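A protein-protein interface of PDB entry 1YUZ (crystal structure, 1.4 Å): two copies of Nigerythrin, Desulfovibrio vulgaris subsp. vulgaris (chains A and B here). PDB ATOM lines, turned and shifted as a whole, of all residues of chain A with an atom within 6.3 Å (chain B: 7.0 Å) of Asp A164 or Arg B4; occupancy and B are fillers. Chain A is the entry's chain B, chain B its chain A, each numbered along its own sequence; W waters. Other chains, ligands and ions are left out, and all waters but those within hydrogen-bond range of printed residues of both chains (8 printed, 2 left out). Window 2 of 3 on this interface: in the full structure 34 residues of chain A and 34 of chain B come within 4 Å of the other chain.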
ATOM      1  N   TYR A  59     -18.602   5.604 -37.626  1.00  0.00           N
ATOM      2  CA  TYR A  59     -18.974   4.610 -36.623  1.00  0.00           C
ATOM      3  C   TYR A  59     -19.791   3.517 -37.305  1.00  0.00           C
ATOM      4  O   TYR A  59     -21.013   3.466 -37.156  1.00  0.00           O
ATOM      5  CB  TYR A  59     -19.818   5.248 -35.517  1.00  0.00           C
ATOM      6  CG  TYR A  59     -19.153   6.381 -34.764  1.00  0.00           C
ATOM      7  CD1 TYR A  59     -19.475   7.711 -35.039  1.00  0.00           C
ATOM      8  CD2 TYR A  59     -18.252   6.122 -33.733  1.00  0.00           C
ATOM      9  CE1 TYR A  59     -18.924   8.754 -34.294  1.00  0.00           C
ATOM     10  CE2 TYR A  59     -17.695   7.155 -32.987  1.00  0.00           C
ATOM     11  CZ  TYR A  59     -18.039   8.466 -33.268  1.00  0.00           C
ATOM     12  OH  TYR A  59     -17.530   9.488 -32.498  1.00  0.00           O
ATOM     13  N   ALA A 159     -22.939   0.764 -26.386  1.00  0.00           N
ATOM     14  CA  ALA A 159     -22.288   1.350 -27.553  1.00  0.00           C
ATOM     15  C   ALA A 159     -21.742   2.733 -27.223  1.00  0.00           C
ATOM     16  O   ALA A 159     -20.686   3.127 -27.714  1.00  0.00           O
ATOM     17  CB  ALA A 159     -23.275   1.440 -28.705  1.00  0.00           C
ATOM     18  N   TYR A 160     -22.467   3.471 -26.388  1.00  0.00           N
ATOM     19  CA  TYR A 160     -22.052   4.808 -25.980  1.00  0.00           C
ATOM     20  C   TYR A 160     -20.783   4.713 -25.133  1.00  0.00           C
ATOM     21  O   TYR A 160     -19.836   5.475 -25.326  1.00  0.00           O
ATOM     22  CB  TYR A 160     -23.179   5.459 -25.173  1.00  0.00           C
ATOM     23  CG  TYR A 160     -22.894   6.853 -24.655  1.00  0.00           C
ATOM     24  CD1 TYR A 160     -23.204   7.981 -25.416  1.00  0.00           C
ATOM     25  CD2 TYR A 160     -22.377   7.045 -23.374  1.00  0.00           C
ATOM     26  CE1 TYR A 160     -23.019   9.263 -24.907  1.00  0.00           C
ATOM     27  CE2 TYR A 160     -22.185   8.322 -22.858  1.00  0.00           C
ATOM     28  CZ  TYR A 160     -22.514   9.422 -23.629  1.00  0.00           C
ATOM     29  OH  TYR A 160     -22.368  10.681 -23.100  1.00  0.00           O
ATOM     30  N   ASN A 161     -20.760   3.769 -24.198  1.00  0.00           N
ATOM     31  CA  ASN A 161     -19.598   3.599 -23.337  1.00  0.00           C
ATOM     32  C   ASN A 161     -18.366   3.165 -24.113  1.00  0.00           C
ATOM     33  O   ASN A 161     -17.245   3.527 -23.756  1.00  0.00           O
ATOM     34  CB  ASN A 161     -19.902   2.591 -22.231  1.00  0.00           C
ATOM     35  CG  ASN A 161     -20.855   3.146 -21.208  1.00  0.00           C
ATOM     36  OD1 ASN A 161     -20.878   4.349 -20.981  1.00  0.00           O
ATOM     37  ND2 ASN A 161     -21.639   2.286 -20.582  1.00  0.00           N
ATOM     38  N   ASP A 162     -18.576   2.398 -25.179  1.00  0.00           N
ATOM     39  CA  ASP A 162     -17.472   1.923 -26.007  1.00  0.00           C
ATOM     40  C   ASP A 162     -17.457   2.610 -27.363  1.00  0.00           C
ATOM     41  O   ASP A 162     -17.006   2.031 -28.351  1.00  0.00           O
ATOM     42  CB  ASP A 162     -17.578   0.413 -26.222  1.00  0.00           C
ATOM     43  CG  ASP A 162     -17.328  -0.369 -24.957  1.00  0.00           C
ATOM     44  OD1 ASP A 162     -16.492   0.085 -24.147  1.00  0.00           O
ATOM     45  OD2 ASP A 162     -17.955  -1.437 -24.781  1.00  0.00           O
ATOM     46  N   ILE A 163     -17.928   3.850 -27.412  1.00  0.00           N
ATOM     47  CA  ILE A 163     -17.987   4.574 -28.671  1.00  0.00           C
ATOM     48  C   ILE A 163     -16.644   4.639 -29.399  1.00  0.00           C
ATOM     49  O   ILE A 163     -16.605   4.643 -30.627  1.00  0.00           O
ATOM     50  CB  ILE A 163     -18.549   6.004 -28.463  1.00  0.00           C
ATOM     51  CG1 ILE A 163     -18.860   6.640 -29.818  1.00  0.00           C
ATOM     52  CG2 ILE A 163     -17.561   6.854 -27.678  1.00  0.00           C
ATOM     53  CD1 ILE A 163     -19.746   7.865 -29.732  1.00  0.00           C
ATOM     54  N   ASP A 164     -15.547   4.670 -28.650  1.00  0.00           N
ATOM     55  CA  ASP A 164     -14.228   4.735 -29.268  1.00  0.00           C
ATOM     56  C   ASP A 164     -13.487   3.403 -29.224  1.00  0.00           C
ATOM     57  O   ASP A 164     -12.277   3.339 -29.464  1.00  0.00           O
ATOM     58  CB  ASP A 164     -13.410   5.840 -28.603  1.00  0.00           C
ATOM     59  CG  ASP A 164     -14.094   7.193 -28.699  1.00  0.00           C
ATOM     60  OD1 ASP A 164     -14.422   7.603 -29.833  1.00  0.00           O
ATOM     61  OD2 ASP A 164     -14.309   7.835 -27.651  1.00  0.00           O
ATOM     62  N   ALA A 165     -14.224   2.338 -28.935  1.00  0.00           N
ATOM     63  CA  ALA A 165     -13.653   1.000 -28.874  1.00  0.00           C
ATOM     64  C   ALA A 165     -14.583   0.001 -29.555  1.00  0.00           C
ATOM     65  O   ALA A 165     -15.058  -0.950 -28.934  1.00  0.00           O
ATOM     66  CB  ALA A 165     -13.417   0.596 -27.425  1.00  0.00           C
ATOM     67  N   PRO A 166     -14.867   0.212 -30.847  1.00  0.00           N
ATOM     68  CA  PRO A 166     -15.751  -0.709 -31.566  1.00  0.00           C
ATOM     69  C   PRO A 166     -15.020  -2.014 -31.861  1.00  0.00           C
ATOM     70  O   PRO A 166     -13.805  -2.107 -31.693  1.00  0.00           O
ATOM     71  CB  PRO A 166     -16.079   0.051 -32.855  1.00  0.00           C
ATOM     72  CG  PRO A 166     -15.742   1.488 -32.543  1.00  0.00           C
ATOM     73  CD  PRO A 166     -14.526   1.373 -31.680  1.00  0.00           C
ATOM     74  N   MET B   1     -17.747  -1.470 -20.341  1.00  0.00           N
ATOM     75  CA  MET B   1     -16.775  -0.512 -20.934  1.00  0.00           C
ATOM     76  C   MET B   1     -15.433  -1.194 -21.161  1.00  0.00           C
ATOM     77  O   MET B   1     -14.816  -1.703 -20.228  1.00  0.00           O
ATOM     78  CB  MET B   1     -16.589   0.689 -20.010  1.00  0.00           C
ATOM     79  CG  MET B   1     -15.675   1.758 -20.576  1.00  0.00           C
ATOM     80  SD  MET B   1     -15.469   3.132 -19.442  1.00  0.00           S
ATOM     81  CE  MET B   1     -14.474   4.234 -20.431  1.00  0.00           C
ATOM     82  N   LYS B   2     -14.986  -1.189 -22.410  1.00  0.00           N
ATOM     83  CA  LYS B   2     -13.728  -1.815 -22.782  1.00  0.00           C
ATOM     84  C   LYS B   2     -12.523  -0.956 -22.423  1.00  0.00           C
ATOM     85  O   LYS B   2     -12.590   0.274 -22.434  1.00  0.00           O
ATOM     86  CB  LYS B   2     -13.736  -2.108 -24.283  1.00  0.00           C
ATOM     87  CG  LYS B   2     -14.868  -3.035 -24.698  1.00  0.00           C
ATOM     88  CD  LYS B   2     -15.153  -2.985 -26.190  1.00  0.00           C
ATOM     89  CE  LYS B   2     -14.003  -3.519 -27.016  1.00  0.00           C
ATOM     90  NZ  LYS B   2     -14.392  -3.588 -28.452  1.00  0.00           N
ATOM     91  N   VAL B   3     -11.420  -1.618 -22.091  1.00  0.00           N
ATOM     92  CA  VAL B   3     -10.190  -0.926 -21.746  1.00  0.00           C
ATOM     93  C   VAL B   3      -9.491  -0.531 -23.041  1.00  0.00           C
ATOM     94  O   VAL B   3      -9.165  -1.388 -23.860  1.00  0.00           O
ATOM     95  CB  VAL B   3      -9.243  -1.834 -20.931  1.00  0.00           C
ATOM     96  CG1 VAL B   3      -7.939  -1.107 -20.647  1.00  0.00           C
ATOM     97  CG2 VAL B   3      -9.916  -2.251 -19.633  1.00  0.00           C
ATOM     98  N   ARG B   4      -9.277   0.768 -23.223  1.00  0.00           N
ATOM     99  CA  ARG B   4      -8.607   1.278 -24.415  1.00  0.00           C
ATOM    100  C   ARG B   4      -7.106   1.304 -24.152  1.00  0.00           C
ATOM    101  O   ARG B   4      -6.666   1.115 -23.018  1.00  0.00           O
ATOM    102  CB  ARG B   4      -9.094   2.697 -24.735  1.00  0.00           C
ATOM    103  CG  ARG B   4     -10.576   2.811 -25.075  1.00  0.00           C
ATOM    104  CD  ARG B   4     -11.007   4.275 -25.147  1.00  0.00           C
ATOM    105  NE  ARG B   4     -10.270   5.025 -26.161  1.00  0.00           N
ATOM    106  CZ  ARG B   4     -10.297   6.348 -26.284  1.00  0.00           C
ATOM    107  NH1 ARG B   4     -11.026   7.082 -25.454  1.00  0.00           N
ATOM    108  NH2 ARG B   4      -9.592   6.940 -27.239  1.00  0.00           N
ATOM    109  N   ALA B   5      -6.322   1.535 -25.199  1.00  0.00           N
ATOM    110  CA  ALA B   5      -4.874   1.597 -25.057  1.00  0.00           C
ATOM    111  C   ALA B   5      -4.510   2.846 -24.265  1.00  0.00           C
ATOM    112  O   ALA B   5      -3.476   2.898 -23.599  1.00  0.00           O
ATOM    113  CB  ALA B   5      -4.212   1.635 -26.431  1.00  0.00           C
ATOM    114  N   GLN B   6      -5.371   3.854 -24.342  1.00  0.00           N
ATOM    115  CA  GLN B   6      -5.150   5.105 -23.629  1.00  0.00           C
ATOM    116  C   GLN B   6      -6.280   5.395 -22.651  1.00  0.00           C
ATOM    117  O   GLN B   6      -7.403   4.914 -22.815  1.00  0.00           O
ATOM    118  CB  GLN B   6      -5.019   6.269 -24.617  1.00  0.00           C
ATOM    119  CG  GLN B   6      -6.102   6.317 -25.681  1.00  0.00           C
ATOM    120  CD  GLN B   6      -5.933   5.240 -26.736  1.00  0.00           C
ATOM    121  OE1 GLN B   6      -4.945   5.225 -27.473  1.00  0.00           O
ATOM    122  NE2 GLN B   6      -6.897   4.328 -26.810  1.00  0.00           N
ATOM    123  N   VAL B   7      -5.969   6.176 -21.622  1.00  0.00           N
ATOM    124  CA  VAL B   7      -6.951   6.553 -20.618  1.00  0.00           C
ATOM    125  C   VAL B   7      -7.916   7.526 -21.290  1.00  0.00           C
ATOM    126  O   VAL B   7      -7.489   8.526 -21.869  1.00  0.00           O
ATOM    127  CB  VAL B   7      -6.268   7.255 -19.426  1.00  0.00           C
ATOM    128  CG1 VAL B   7      -7.279   7.526 -18.332  1.00  0.00           C
ATOM    129  CG2 VAL B   7      -5.131   6.395 -18.898  1.00  0.00           C
ATOM    130  N   PRO B   8      -9.230   7.249 -21.231  1.00  0.00           N
ATOM    131  CA  PRO B   8     -10.194   8.152 -21.864  1.00  0.00           C
ATOM    132  C   PRO B   8     -10.226   9.555 -21.267  1.00  0.00           C
ATOM    133  O   PRO B   8     -10.225   9.733 -20.049  1.00  0.00           O
ATOM    134  CB  PRO B   8     -11.521   7.409 -21.704  1.00  0.00           C
ATOM    135  CG  PRO B   8     -11.321   6.633 -20.440  1.00  0.00           C
ATOM    136  CD  PRO B   8      -9.914   6.112 -20.590  1.00  0.00           C
ATOM    137  N   THR B   9     -10.244  10.553 -22.143  1.00  0.00           N
ATOM    138  CA  THR B   9     -10.280  11.947 -21.726  1.00  0.00           C
ATOM    139  C   THR B   9     -11.154  12.728 -22.696  1.00  0.00           C
ATOM    140  O   THR B   9     -11.529  12.223 -23.755  1.00  0.00           O
ATOM    141  CB  THR B   9      -8.878  12.581 -21.746  1.00  0.00           C
ATOM    142  OG1 THR B   9      -8.404  12.622 -23.097  1.00  0.00           O
ATOM    143  CG2 THR B   9      -7.908  11.776 -20.887  1.00  0.00           C
ATOM    144  N   ASN B  12      -9.401  12.732 -26.137  1.00  0.00           N
ATOM    145  CA  ASN B  12      -9.344  11.576 -27.028  1.00  0.00           C
ATOM    146  C   ASN B  12     -10.631  10.768 -27.169  1.00  0.00           C
ATOM    147  O   ASN B  12     -10.638   9.743 -27.851  1.00  0.00           O
ATOM    148  CB  ASN B  12      -8.219  10.625 -26.600  1.00  0.00           C
ATOM    149  CG  ASN B  12      -8.491   9.953 -25.262  1.00  0.00           C
ATOM    150  OD1 ASN B  12      -9.643   9.781 -24.860  1.00  0.00           O
ATOM    151  ND2 ASN B  12      -7.428   9.549 -24.575  1.00  0.00           N
ATOM    152  N   ALA B  13     -11.710  11.220 -26.535  1.00  0.00           N
ATOM    153  CA  ALA B  13     -12.984  10.500 -26.597  1.00  0.00           C
ATOM    154  C   ALA B  13     -14.035  11.257 -27.400  1.00  0.00           C
ATOM    155  O   ALA B  13     -13.954  12.475 -27.552  1.00  0.00           O
ATOM    156  CB  ALA B  13     -13.497  10.235 -25.187  1.00  0.00           C
ATOM    157  N   THR B  14     -15.034  10.542 -27.906  1.00  0.00           N
ATOM    158  CA  THR B  14     -16.063  11.195 -28.700  1.00  0.00           C
ATOM    159  C   THR B  14     -17.470  11.138 -28.112  1.00  0.00           C
ATOM    160  O   THR B  14     -18.451  11.324 -28.828  1.00  0.00           O
ATOM    161  CB  THR B  14     -16.080  10.645 -30.146  1.00  0.00           C
ATOM    162  OG1 THR B  14     -16.384   9.247 -30.130  1.00  0.00           O
ATOM    163  CG2 THR B  14     -14.716  10.857 -30.811  1.00  0.00           C
ATOM    164  N   ASN B  15     -17.574  10.871 -26.814  1.00  0.00           N
ATOM    165  CA  ASN B  15     -18.887  10.858 -26.177  1.00  0.00           C
ATOM    166  C   ASN B  15     -18.966  11.921 -25.085  1.00  0.00           C
ATOM    167  O   ASN B  15     -19.567  11.715 -24.031  1.00  0.00           O
ATOM    168  CB  ASN B  15     -19.238   9.460 -25.628  1.00  0.00           C
ATOM    169  CG  ASN B  15     -18.215   8.922 -24.641  1.00  0.00           C
ATOM    170  OD1 ASN B  15     -17.167   9.520 -24.408  1.00  0.00           O
ATOM    171  ND2 ASN B  15     -18.524   7.771 -24.055  1.00  0.00           N
ATOM    172  N   PHE B  16     -18.364  13.075 -25.357  1.00  0.00           N
ATOM    173  CA  PHE B  16     -18.369  14.180 -24.410  1.00  0.00           C
ATOM    174  C   PHE B  16     -19.222  15.362 -24.851  1.00  0.00           C
ATOM    175  O   PHE B  16     -19.145  16.438 -24.264  1.00  0.00           O
ATOM    176  CB  PHE B  16     -16.941  14.655 -24.129  1.00  0.00           C
ATOM    177  CG  PHE B  16     -16.210  13.802 -23.131  1.00  0.00           C
ATOM    178  CD1 PHE B  16     -15.795  12.519 -23.464  1.00  0.00           C
ATOM    179  CD2 PHE B  16     -15.960  14.272 -21.847  1.00  0.00           C
ATOM    180  CE1 PHE B  16     -15.142  11.713 -22.533  1.00  0.00           C
ATOM    181  CE2 PHE B  16     -15.308  13.471 -20.907  1.00  0.00           C
ATOM    182  CZ  PHE B  16     -14.900  12.191 -21.254  1.00  0.00           C
ATOM    183  N   LYS B 188      -8.183  -4.455 -15.127  1.00  0.00           N
ATOM    184  CA  LYS B 188      -8.020  -3.119 -14.583  1.00  0.00           C
ATOM    185  C   LYS B 188      -9.179  -2.206 -14.951  1.00  0.00           C
ATOM    186  O   LYS B 188     -10.012  -2.541 -15.791  1.00  0.00           O
ATOM    187  CB  LYS B 188      -6.710  -2.506 -15.082  1.00  0.00           C
ATOM    188  CG  LYS B 188      -6.642  -2.318 -16.589  1.00  0.00           C
ATOM    189  CD  LYS B 188      -5.333  -1.656 -16.997  1.00  0.00           C
ATOM    190  CE  LYS B 188      -5.256  -1.460 -18.501  1.00  0.00           C
ATOM    191  NZ  LYS B 188      -3.981  -0.803 -18.908  1.00  0.00           N
ATOM    192  N   PRO B 190     -11.100   0.633 -16.748  1.00  0.00           N
ATOM    193  CA  PRO B 190     -10.982   1.256 -18.070  1.00  0.00           C
ATOM    194  C   PRO B 190     -10.977   2.781 -18.017  1.00  0.00           C
ATOM    195  O   PRO B 190     -10.668   3.441 -19.009  1.00  0.00           O
ATOM    196  CB  PRO B 190     -12.193   0.707 -18.814  1.00  0.00           C
ATOM    197  CG  PRO B 190     -13.214   0.615 -17.726  1.00  0.00           C
ATOM    198  CD  PRO B 190     -12.422   0.005 -16.582  1.00  0.00           C
ATOM    199  N   PHE B 193      -7.352   2.986 -15.032  1.00  0.00           N
ATOM    200  CA  PHE B 193      -6.341   1.931 -15.118  1.00  0.00           C
ATOM    201  C   PHE B 193      -5.925   1.244 -13.817  1.00  0.00           C
ATOM    202  O   PHE B 193      -4.997   0.437 -13.817  1.00  0.00           O
ATOM    203  CB  PHE B 193      -5.095   2.460 -15.840  1.00  0.00           C
ATOM    204  CG  PHE B 193      -5.236   2.522 -17.340  1.00  0.00           C
ATOM    205  CD1 PHE B 193      -6.490   2.468 -17.944  1.00  0.00           C
ATOM    206  CD2 PHE B 193      -4.111   2.652 -18.148  1.00  0.00           C
ATOM    207  CE1 PHE B 193      -6.621   2.542 -19.330  1.00  0.00           C
ATOM    208  CE2 PHE B 193      -4.232   2.727 -19.535  1.00  0.00           C
ATOM    209  CZ  PHE B 193      -5.487   2.672 -20.127  1.00  0.00           C
HETATM  210  O   HOH W   1     -13.769   6.670 -25.268  1.00  0.00           O
HETATM  211  O   HOH W   2     -19.813  -0.859 -22.703  1.00  0.00           O
HETATM  212  O   HOH W   3     -18.038  -3.141 -22.640  1.00  0.00           O
HETATM  213  O   HOH W   4     -19.931  -0.308 -19.256  1.00  0.00           O
HETATM  214  O   HOH W   5     -19.787  11.144 -31.271  1.00  0.00           O
HETATM  215  O   HOH W   6     -17.791   5.406 -19.787  1.00  0.00           O
HETATM  216  O   HOH W   7     -22.766  12.619 -24.873  1.00  0.00           O
HETATM  217  O   HOH W   8     -16.945   5.946 -22.320  1.00  0.00           O
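Of the printed residues of chain B, Asp A162 touches Met B1 (3.3 Å) and Lys B2 (2.6 Å).
Printed residues of chain B within 4 Å of Ile A163: Thr B14 and Asn B15.
Printed residues of chain B within 4 Å of Ala A165: Lys B2 (2.8 Å).
Printed residues of chain A within 4 Å of Ala B13: Asp A164.
The nearest printed residue of chain B that does not touch Asn A161 is Asn B15 (4.4 Å).
Of the 17 printed residues of chain B, 6 touch a printed residue of chain A.
Of the 9 printed residues of chain A, 8 touch a printed residue of chain B.
Printed residues of chain A that touch a printed residue of chain B: Tyr A59, Tyr A160, Asn A161, Asp A162, Ile A163, Asp A164, Ala A165 and Pro A166.
Hydrophobic or aromatic side chains of chain A within 4 Å of the printed part of chain B: Tyr A59, Tyr A160 and Ile A163.
Among the printed residues, no Asp or Glu carboxylate lies within 4 Å of a Lys or Arg side-chain nitrogen of the other chain.
The side-chain hydroxyl of Thr B14 sits at hydrogen-bond distance from the side-chain hydroxyl of Tyr A59 (2.6 Å).
OG1 of Thr B14 sits at hydrogen-bond distance from OD1 of Asp A164 (2.6 Å).
The side-chain amino group (NZ) of Lys B2 sits at hydrogen-bond distance from the backbone carbonyl oxygen (O) of Ala A165 (2.8 Å).
O of Tyr A160 lies within hydrogen-bond range of ND2 of Asn B15, 2.9 Å away.
The backbone NH of Lys B2 sits at hydrogen-bond distance from the side-chain carboxylate of Asp A162 (2.6 Å).
Water W7 bridges the side-chain hydroxyl of Tyr A160 (2.7 Å) and the backbone carbonyl oxygen of Asn B15 (3.4 Å).
Water W4 bridges the backbone NH (N) of Met B1 and the side-chain amide nitrogen (ND2) of Asn A161.
Water W1 lies within hydrogen-bond range of the side-chain carboxylate (OD2) of Asp A164 and the guanidinium group (NH1) of Arg B4.
Water W3 lies within hydrogen-bond range of OD2 of Asp A162 and N of Met B1.
Water W2 lies within hydrogen-bond range of OD2 of Asp A162 (2.8 Å) and N of Met B1 (3.2 Å).
Water W6 lies within hydrogen-bond range of the side-chain sulfur of Met B1 (3.3 Å) and the side-chain amide oxygen of Asn A161 (3.5 Å).
Asn A161 touches Met B1.
Met B1 touches Asp A162 (CA to OD1, 3.3 Å).
Thr B14 touches Ile A163.
Ile A163 touches Asn B15 (CG2 to CB, 3.7 Å).
CB of Asp A164 touches CZ of Arg B4, 3.9 Å away.
Asp A164 touches Ala B13 (OD2 to CA, 3.2 Å).
Lys B2 touches Pro A166 (NZ to O, 3.6 Å).
No position is printed for both chains.
Of the 12 pairs that touch across the chains among the printed residues, none has its exchanged pair printed and touching as well.
NH2 of Arg B4 is in hydrogen-bond range of O of Asn B12.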
